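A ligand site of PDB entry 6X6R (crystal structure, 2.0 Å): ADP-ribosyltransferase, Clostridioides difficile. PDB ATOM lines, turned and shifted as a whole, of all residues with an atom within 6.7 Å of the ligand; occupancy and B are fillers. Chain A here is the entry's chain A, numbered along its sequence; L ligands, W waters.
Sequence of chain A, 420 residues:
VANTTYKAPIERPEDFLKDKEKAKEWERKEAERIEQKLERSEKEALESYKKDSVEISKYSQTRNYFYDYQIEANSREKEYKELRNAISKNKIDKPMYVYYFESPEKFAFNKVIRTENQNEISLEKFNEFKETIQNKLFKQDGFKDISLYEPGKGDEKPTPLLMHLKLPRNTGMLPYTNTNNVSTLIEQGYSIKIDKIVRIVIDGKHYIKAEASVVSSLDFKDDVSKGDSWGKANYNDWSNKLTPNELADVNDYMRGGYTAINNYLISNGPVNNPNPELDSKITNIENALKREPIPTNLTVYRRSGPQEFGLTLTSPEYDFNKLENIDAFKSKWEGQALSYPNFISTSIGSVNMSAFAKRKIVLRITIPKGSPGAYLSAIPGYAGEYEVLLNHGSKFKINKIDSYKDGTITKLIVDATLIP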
ATOM      1  N   TYR A 301      -6.417  -0.615   2.948  1.00  0.00           N
ATOM      2  CA  TYR A 301      -5.981  -0.117   1.659  1.00  0.00           C
ATOM      3  C   TYR A 301      -6.796  -0.641   0.529  1.00  0.00           C
ATOM      4  O   TYR A 301      -7.020  -1.829   0.426  1.00  0.00           O
ATOM      5  CB  TYR A 301      -4.501  -0.476   1.460  1.00  0.00           C
ATOM      6  CG  TYR A 301      -3.633   0.206   2.483  1.00  0.00           C
ATOM      7  CD1 TYR A 301      -3.407  -0.380   3.738  1.00  0.00           C
ATOM      8  CD2 TYR A 301      -3.108   1.472   2.248  1.00  0.00           C
ATOM      9  CE1 TYR A 301      -2.672   0.285   4.718  1.00  0.00           C
ATOM     10  CE2 TYR A 301      -2.322   2.114   3.194  1.00  0.00           C
ATOM     11  CZ  TYR A 301      -2.128   1.528   4.432  1.00  0.00           C
ATOM     12  OH  TYR A 301      -1.367   2.181   5.366  1.00  0.00           O
ATOM     13  N   ARG A 302      -7.231   0.253  -0.352  1.00  0.00           N
ATOM     14  CA  ARG A 302      -7.966  -0.194  -1.523  1.00  0.00           C
ATOM     15  C   ARG A 302      -7.271   0.349  -2.765  1.00  0.00           C
ATOM     16  O   ARG A 302      -6.975   1.546  -2.834  1.00  0.00           O
ATOM     17  CB  ARG A 302      -9.472   0.208  -1.445  1.00  0.00           C
ATOM     18  CG  ARG A 302     -10.210  -0.070  -2.731  1.00  0.00           C
ATOM     19  CD  ARG A 302     -11.682   0.231  -2.670  1.00  0.00           C
ATOM     20  NE  ARG A 302     -12.244   0.058  -4.010  1.00  0.00           N
ATOM     21  CZ  ARG A 302     -12.615  -1.100  -4.534  1.00  0.00           C
ATOM     22  NH1 ARG A 302     -12.549  -2.215  -3.812  1.00  0.00           N
ATOM     23  NH2 ARG A 302     -13.059  -1.155  -5.783  1.00  0.00           N
ATOM     24  N   ARG A 303      -7.025  -0.507  -3.734  1.00  0.00           N
ATOM     25  CA  ARG A 303      -6.472  -0.108  -5.019  1.00  0.00           C
ATOM     26  C   ARG A 303      -7.693   0.204  -5.860  1.00  0.00           C
ATOM     27  O   ARG A 303      -8.477  -0.698  -6.173  1.00  0.00           O
ATOM     28  CB  ARG A 303      -5.637  -1.243  -5.638  1.00  0.00           C
ATOM     29  CG  ARG A 303      -4.367  -1.511  -4.841  1.00  0.00           C
ATOM     30  CD  ARG A 303      -3.188  -0.652  -5.288  1.00  0.00           C
ATOM     31  NE  ARG A 303      -2.142  -0.695  -4.264  1.00  0.00           N
ATOM     32  CZ  ARG A 303      -0.890  -0.306  -4.430  1.00  0.00           C
ATOM     33  NH1 ARG A 303      -0.469   0.108  -5.612  1.00  0.00           N
ATOM     34  NH2 ARG A 303      -0.047  -0.341  -3.410  1.00  0.00           N
ATOM     35  N   SER A 304      -7.922   1.489  -6.117  1.00  0.00           N
ATOM     36  CA  SER A 304      -9.111   1.956  -6.818  1.00  0.00           C
ATOM     37  C   SER A 304      -8.891   2.122  -8.300  1.00  0.00           C
ATOM     38  O   SER A 304      -7.844   2.618  -8.728  1.00  0.00           O
ATOM     39  CB  SER A 304      -9.589   3.285  -6.238  1.00  0.00           C
ATOM     40  OG  SER A 304      -9.955   3.145  -4.877  1.00  0.00           O
ATOM     41  N   GLY A 305      -9.909   1.733  -9.049  1.00  0.00           N
ATOM     42  CA  GLY A 305      -9.966   1.908 -10.497  1.00  0.00           C
ATOM     43  C   GLY A 305     -10.359   3.366 -10.767  1.00  0.00           C
ATOM     44  O   GLY A 305     -10.897   4.027  -9.877  1.00  0.00           O
ATOM     45  N   GLU A 308     -14.138   4.885  -9.812  1.00  0.00           N
ATOM     46  CA  GLU A 308     -14.493   5.216  -8.432  1.00  0.00           C
ATOM     47  C   GLU A 308     -14.314   6.729  -8.208  1.00  0.00           C
ATOM     48  O   GLU A 308     -14.902   7.285  -7.275  1.00  0.00           O
ATOM     49  CB  GLU A 308     -13.645   4.382  -7.467  1.00  0.00           C
ATOM     50  CG  GLU A 308     -13.916   2.892  -7.602  1.00  0.00           C
ATOM     51  CD  GLU A 308     -12.931   1.995  -6.873  1.00  0.00           C
ATOM     52  OE1 GLU A 308     -12.690   2.246  -5.673  1.00  0.00           O
ATOM     53  OE2 GLU A 308     -12.421   1.041  -7.504  1.00  0.00           O
ATOM     54  N   SER A 345     -14.527  -3.751  -0.924  1.00  0.00           N
ATOM     55  CA  SER A 345     -13.421  -4.630  -0.532  1.00  0.00           C
ATOM     56  C   SER A 345     -12.161  -3.827  -0.375  1.00  0.00           C
ATOM     57  O   SER A 345     -11.880  -2.931  -1.167  1.00  0.00           O
ATOM     58  CB  SER A 345     -13.217  -5.738  -1.553  1.00  0.00           C
ATOM     59  OG  SER A 345     -14.008  -6.841  -1.154  1.00  0.00           O
ATOM     60  N   THR A 346     -11.381  -4.145   0.672  1.00  0.00           N
ATOM     61  CA  THR A 346     -10.111  -3.497   0.985  1.00  0.00           C
ATOM     62  C   THR A 346      -9.116  -4.550   1.497  1.00  0.00           C
ATOM     63  O   THR A 346      -9.544  -5.665   1.776  1.00  0.00           O
ATOM     64  CB  THR A 346     -10.329  -2.442   2.083  1.00  0.00           C
ATOM     65  OG1 THR A 346     -10.599  -3.089   3.327  1.00  0.00           O
ATOM     66  CG2 THR A 346     -11.431  -1.415   1.750  1.00  0.00           C
ATOM     67  N   SER A 347      -7.805  -4.214   1.604  1.00  0.00           N
ATOM     68  CA  SER A 347      -6.783  -5.125   2.180  1.00  0.00           C
ATOM     69  C   SER A 347      -6.227  -4.554   3.489  1.00  0.00           C
ATOM     70  O   SER A 347      -6.141  -3.334   3.623  1.00  0.00           O
ATOM     71  CB  SER A 347      -5.619  -5.354   1.229  1.00  0.00           C
ATOM     72  OG  SER A 347      -6.013  -6.001   0.033  1.00  0.00           O
ATOM     73  N   GLY A 349      -3.250  -4.787   4.127  1.00  0.00           N
ATOM     74  CA  GLY A 349      -1.928  -4.419   3.680  1.00  0.00           C
ATOM     75  C   GLY A 349      -1.944  -3.453   2.517  1.00  0.00           C
ATOM     76  O   GLY A 349      -2.851  -3.482   1.683  1.00  0.00           O
ATOM     77  N   VAL A 351       0.599  -3.198   0.198  1.00  0.00           N
ATOM     78  CA  VAL A 351       1.411  -3.664  -0.936  1.00  0.00           C
ATOM     79  C   VAL A 351       0.625  -3.706  -2.254  1.00  0.00           C
ATOM     80  O   VAL A 351      -0.599  -3.893  -2.258  1.00  0.00           O
ATOM     81  CB  VAL A 351       2.129  -5.023  -0.671  1.00  0.00           C
ATOM     82  CG1 VAL A 351       3.154  -4.877   0.451  1.00  0.00           C
ATOM     83  CG2 VAL A 351       1.142  -6.169  -0.387  1.00  0.00           C
ATOM     84  N   MET A 353      -0.373  -5.594  -5.754  1.00  0.00           N
ATOM     85  CA  MET A 353      -0.733  -6.975  -6.033  1.00  0.00           C
ATOM     86  C   MET A 353      -0.975  -7.063  -7.513  1.00  0.00           C
ATOM     87  O   MET A 353      -1.407  -6.087  -8.092  1.00  0.00           O
ATOM     88  CB  MET A 353      -1.992  -7.374  -5.266  1.00  0.00           C
ATOM     89  CG  MET A 353      -1.723  -7.616  -3.791  1.00  0.00           C
ATOM     90  SD  MET A 353      -3.211  -7.680  -2.782  1.00  0.00           S
ATOM     91  CE  MET A 353      -3.751  -5.879  -2.854  1.00  0.00           C
ATOM     92  N   SER A 354      -0.671  -8.221  -8.127  1.00  0.00           N
ATOM     93  CA  SER A 354      -0.819  -8.436  -9.569  1.00  0.00           C
ATOM     94  C   SER A 354      -2.191  -8.020 -10.090  1.00  0.00           C
ATOM     95  O   SER A 354      -2.264  -7.358 -11.110  1.00  0.00           O
ATOM     96  CB  SER A 354      -0.542  -9.890  -9.938  1.00  0.00           C
ATOM     97  OG  SER A 354       0.740 -10.321  -9.501  1.00  0.00           O
ATOM     98  N   ALA A 355      -3.264  -8.377  -9.369  1.00  0.00           N
ATOM     99  CA  ALA A 355      -4.657  -8.060  -9.721  1.00  0.00           C
ATOM    100  C   ALA A 355      -4.896  -6.557  -9.901  1.00  0.00           C
ATOM    101  O   ALA A 355      -5.772  -6.173 -10.673  1.00  0.00           O
ATOM    102  CB  ALA A 355      -5.593  -8.606  -8.644  1.00  0.00           C
ATOM    103  N   PHE A 356      -4.121  -5.693  -9.200  1.00  0.00           N
ATOM    104  CA  PHE A 356      -4.301  -4.241  -9.188  1.00  0.00           C
ATOM    105  C   PHE A 356      -3.059  -3.478  -9.584  1.00  0.00           C
ATOM    106  O   PHE A 356      -2.972  -2.290  -9.281  1.00  0.00           O
ATOM    107  CB  PHE A 356      -4.749  -3.791  -7.794  1.00  0.00           C
ATOM    108  CG  PHE A 356      -5.802  -4.650  -7.161  1.00  0.00           C
ATOM    109  CD1 PHE A 356      -7.041  -4.821  -7.770  1.00  0.00           C
ATOM    110  CD2 PHE A 356      -5.556  -5.296  -5.955  1.00  0.00           C
ATOM    111  CE1 PHE A 356      -8.002  -5.671  -7.219  1.00  0.00           C
ATOM    112  CE2 PHE A 356      -6.513  -6.154  -5.410  1.00  0.00           C
ATOM    113  CZ  PHE A 356      -7.721  -6.354  -6.052  1.00  0.00           C
ATOM    114  N   ARG A 359      -3.557   0.000 -11.221  1.00  0.00           N
ATOM    115  CA  ARG A 359      -4.456   0.981 -10.606  1.00  0.00           C
ATOM    116  C   ARG A 359      -3.636   2.119 -10.004  1.00  0.00           C
ATOM    117  O   ARG A 359      -2.639   1.881  -9.324  1.00  0.00           O
ATOM    118  CB  ARG A 359      -5.404   0.343  -9.602  1.00  0.00           C
ATOM    119  CG  ARG A 359      -6.323  -0.658 -10.260  1.00  0.00           C
ATOM    120  CD  ARG A 359      -7.429  -1.041  -9.339  1.00  0.00           C
ATOM    121  NE  ARG A 359      -8.251  -2.080  -9.943  1.00  0.00           N
ATOM    122  CZ  ARG A 359      -9.368  -2.559  -9.423  1.00  0.00           C
ATOM    123  NH1 ARG A 359      -9.837  -2.074  -8.273  1.00  0.00           N
ATOM    124  NH2 ARG A 359     -10.039  -3.513 -10.042  1.00  0.00           N
ATOM    125  N   SER A 377     -11.070 -12.867   4.814  1.00  0.00           N
ATOM    126  CA  SER A 377      -9.978 -13.830   4.626  1.00  0.00           C
ATOM    127  C   SER A 377      -9.801 -14.836   5.783  1.00  0.00           C
ATOM    128  O   SER A 377      -9.004 -15.764   5.636  1.00  0.00           O
ATOM    129  CB  SER A 377      -8.667 -13.113   4.320  1.00  0.00           C
ATOM    130  OG  SER A 377      -8.803 -12.482   3.061  1.00  0.00           O
ATOM    131  N   TYR A 382     -12.698 -19.961   1.655  1.00  0.00           N
ATOM    132  CA  TYR A 382     -12.448 -18.815   0.800  1.00  0.00           C
ATOM    133  C   TYR A 382     -10.961 -18.592   0.496  1.00  0.00           C
ATOM    134  O   TYR A 382     -10.144 -18.516   1.421  1.00  0.00           O
ATOM    135  CB  TYR A 382     -13.085 -17.545   1.388  1.00  0.00           C
ATOM    136  CG  TYR A 382     -12.960 -16.310   0.536  1.00  0.00           C
ATOM    137  CD1 TYR A 382     -13.553 -16.234  -0.728  1.00  0.00           C
ATOM    138  CD2 TYR A 382     -12.318 -15.171   1.021  1.00  0.00           C
ATOM    139  CE1 TYR A 382     -13.463 -15.082  -1.504  1.00  0.00           C
ATOM    140  CE2 TYR A 382     -12.280 -13.991   0.271  1.00  0.00           C
ATOM    141  CZ  TYR A 382     -12.839 -13.956  -0.988  1.00  0.00           C
ATOM    142  OH  TYR A 382     -12.763 -12.824  -1.760  1.00  0.00           O
ATOM    143  N   ALA A 383     -10.631 -18.470  -0.798  1.00  0.00           N
ATOM    144  CA  ALA A 383      -9.292 -18.247  -1.319  1.00  0.00           C
ATOM    145  C   ALA A 383      -8.783 -16.809  -1.129  1.00  0.00           C
ATOM    146  O   ALA A 383      -7.630 -16.663  -0.704  1.00  0.00           O
ATOM    147  CB  ALA A 383      -9.218 -18.651  -2.791  1.00  0.00           C
ATOM    148  N   GLY A 384      -9.604 -15.804  -1.433  1.00  0.00           N
ATOM    149  CA  GLY A 384      -9.281 -14.376  -1.308  1.00  0.00           C
ATOM    150  C   GLY A 384      -8.434 -14.013  -0.100  1.00  0.00           C
ATOM    151  O   GLY A 384      -8.649 -14.541   1.003  1.00  0.00           O
ATOM    152  N   GLU A 385      -7.447 -13.116  -0.280  1.00  0.00           N
ATOM    153  CA  GLU A 385      -6.498 -12.837   0.804  1.00  0.00           C
ATOM    154  C   GLU A 385      -6.485 -11.399   1.296  1.00  0.00           C
ATOM    155  O   GLU A 385      -6.704 -10.458   0.517  1.00  0.00           O
ATOM    156  CB  GLU A 385      -5.061 -13.286   0.411  1.00  0.00           C
ATOM    157  CG  GLU A 385      -4.928 -14.750  -0.018  1.00  0.00           C
ATOM    158  CD  GLU A 385      -4.256 -15.722   0.937  1.00  0.00           C
ATOM    159  OE1 GLU A 385      -3.121 -15.428   1.390  1.00  0.00           O
ATOM    160  OE2 GLU A 385      -4.847 -16.792   1.214  1.00  0.00           O
ATOM    161  N   TYR A 386      -6.253 -11.246   2.628  1.00  0.00           N
ATOM    162  CA  TYR A 386      -6.055  -9.983   3.382  1.00  0.00           C
ATOM    163  C   TYR A 386      -7.264  -9.048   3.355  1.00  0.00           C
ATOM    164  O   TYR A 386      -7.166  -7.862   3.688  1.00  0.00           O
ATOM    165  CB  TYR A 386      -4.789  -9.258   2.844  1.00  0.00           C
ATOM    166  CG  TYR A 386      -3.572 -10.150   2.708  1.00  0.00           C
ATOM    167  CD1 TYR A 386      -3.112 -10.899   3.782  1.00  0.00           C
ATOM    168  CD2 TYR A 386      -2.908 -10.272   1.493  1.00  0.00           C
ATOM    169  CE1 TYR A 386      -2.024 -11.755   3.656  1.00  0.00           C
ATOM    170  CE2 TYR A 386      -1.825 -11.142   1.348  1.00  0.00           C
ATOM    171  CZ  TYR A 386      -1.370 -11.875   2.432  1.00  0.00           C
ATOM    172  OH  TYR A 386      -0.297 -12.718   2.338  1.00  0.00           O
ATOM    173  N   GLU A 387      -8.431  -9.594   3.033  1.00  0.00           N
ATOM    174  CA  GLU A 387      -9.633  -8.837   2.765  1.00  0.00           C
ATOM    175  C   GLU A 387     -10.519  -8.495   3.959  1.00  0.00           C
ATOM    176  O   GLU A 387     -10.949  -9.385   4.702  1.00  0.00           O
ATOM    177  CB  GLU A 387     -10.428  -9.640   1.719  1.00  0.00           C
ATOM    178  CG  GLU A 387     -11.633  -8.966   1.091  1.00  0.00           C
ATOM    179  CD  GLU A 387     -12.176  -9.798  -0.066  1.00  0.00           C
ATOM    180  OE1 GLU A 387     -13.129  -9.344  -0.737  1.00  0.00           O
ATOM    181  OE2 GLU A 387     -11.646 -10.908  -0.300  1.00  0.00           O
ATOM    182  N   VAL A 388     -10.791  -7.178   4.099  1.00  0.00           N
ATOM    183  CA  VAL A 388     -11.769  -6.562   5.000  1.00  0.00           C
ATOM    184  C   VAL A 388     -12.914  -6.036   4.092  1.00  0.00           C
ATOM    185  O   VAL A 388     -12.664  -5.236   3.181  1.00  0.00           O
ATOM    186  CB  VAL A 388     -11.198  -5.434   5.876  1.00  0.00           C
ATOM    187  CG1 VAL A 388     -12.317  -4.616   6.556  1.00  0.00           C
ATOM    188  CG2 VAL A 388     -10.194  -5.983   6.902  1.00  0.00           C
HETATM  189  N1  LIG L   1      -7.867  -3.253  -3.481  1.00  0.00           N
HETATM  190 CL1  LIG L   1      -1.533 -13.767  -1.181  1.00  0.00          CL
HETATM  191  C1  LIG L   1      -7.180  -3.921  -2.532  1.00  0.00           C
HETATM  192  N2  LIG L   1      -7.559  -5.123  -2.067  1.00  0.00           N
HETATM  193  C2  LIG L   1      -8.718  -5.660  -2.478  1.00  0.00           C
HETATM  194  C3  LIG L   1      -9.535  -5.042  -3.535  1.00  0.00           C
HETATM  195  C4  LIG L   1      -8.997  -3.749  -4.060  1.00  0.00           C
HETATM  196  N3  LIG L   1      -9.625  -3.036  -5.029  1.00  0.00           N
HETATM  197  N4  LIG L   1     -10.499  -5.942  -3.849  1.00  0.00           N
HETATM  198  C5  LIG L   1     -10.383  -7.077  -3.067  1.00  0.00           C
HETATM  199  C6  LIG L   1      -9.281  -7.003  -2.221  1.00  0.00           C
HETATM  200  C7  LIG L   1      -6.837  -8.756  -2.616  1.00  0.00           C
HETATM  201  N5  LIG L   1      -7.952  -9.116  -1.715  1.00  0.00           N
HETATM  202  C8  LIG L   1      -8.797  -8.010  -1.192  1.00  0.00           C
HETATM  203  C9  LIG L   1      -2.588 -13.038  -2.445  1.00  0.00           C
HETATM  204  C10 LIG L   1      -3.644 -13.787  -2.971  1.00  0.00           C
HETATM  205  C11 LIG L   1      -4.484 -13.226  -3.928  1.00  0.00           C
HETATM  206  C12 LIG L   1      -8.725 -10.207  -2.346  1.00  0.00           C
HETATM  207  C13 LIG L   1      -7.756 -10.892  -3.319  1.00  0.00           C
HETATM  208  O1  LIG L   1      -7.394 -12.195  -2.864  1.00  0.00           O
HETATM  209  C14 LIG L   1      -6.511 -10.042  -3.364  1.00  0.00           C
HETATM  210  C15 LIG L   1      -6.004  -9.788  -4.793  1.00  0.00           C
HETATM  211  S1  LIG L   1      -5.313 -11.251  -5.534  1.00  0.00           S
HETATM  212  C16 LIG L   1      -4.249 -11.913  -4.373  1.00  0.00           C
HETATM  213  C17 LIG L   1      -3.182 -11.164  -3.861  1.00  0.00           C
HETATM  214  C18 LIG L   1      -2.351 -11.729  -2.882  1.00  0.00           C
HETATM  215  O   HOH W   1      -3.093 -10.251  -7.316  1.00  0.00           O
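OG of Ser 347 sits at hydrogen-bond distance from N2 of the ligand, 2.8 Å away. The backbone carbonyl oxygen (O) of Glu 385 lies close to a nitrogen (N5) of the ligand. The backbone carbonyl oxygen (O) of Arg 303 lies within hydrogen-bond range of a nitrogen (N3) of the ligand, 2.8 Å away. A nitrogen (N1) of the ligand lies within hydrogen-bond range of the backbone NH (N) of Arg 303 (2.9 Å). O1 of the ligand lies within hydrogen-bond range of N of Glu 385 (2.7 Å).
The guanidinium group (NH1) of Arg 302 is in hydrogen-bond range of the backbone carbonyl oxygen (O) of Ser 345, 2.8 Å away. OE1 of Glu 308 lies within salt-bridge range of NE of Arg 302. The side-chain hydroxyl (OG) of Ser 377 is in hydrogen-bond range of the backbone NH (N) of Glu 387. O of Val 388 is in hydrogen-bond range of OG1 of Thr 346, at 3.0 Å. The backbone NH (N) of Ser 347 lies within hydrogen-bond range of the backbone carbonyl oxygen (O) of Tyr 301 (2.8 Å). The guanidinium group (NH1) of Arg 359 sits at hydrogen-bond distance from the backbone carbonyl oxygen (O) of Arg 303, at 2.9 Å. N of Tyr 386 is in hydrogen-bond range of OG of Ser 377, 2.9 Å away. The backbone carbonyl oxygen of Gly 384 sits at hydrogen-bond distance from the side-chain hydroxyl of Ser 377 (2.9 Å).
NH1 of Arg 302 sits close to N3 of the ligand (3.3 Å). N3 of the ligand lies close to NH1 of Arg 359 (3.4 Å). Merely in contact with the ligand: Tyr 301, Ser 345, Thr 346, Met 353, Phe 356, Gly 384, Tyr 386 and Glu 387. Hydrophobic or aromatic side chains within 4 Å of the ligand: Met 353, Phe 356 and Tyr 386. Along chain A the residues within 4 Å of the ligand span positions 301 to 387. The nearest printed residue that does not touch the ligand is Ala 355 (4.05 Å).
Water W1 lies within hydrogen-bond range of the backbone NH of Ala 355 (2.8 Å), a sulfur (S1) of the ligand (3.0 Å) and the backbone NH of Ser 354 (3.3 Å).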
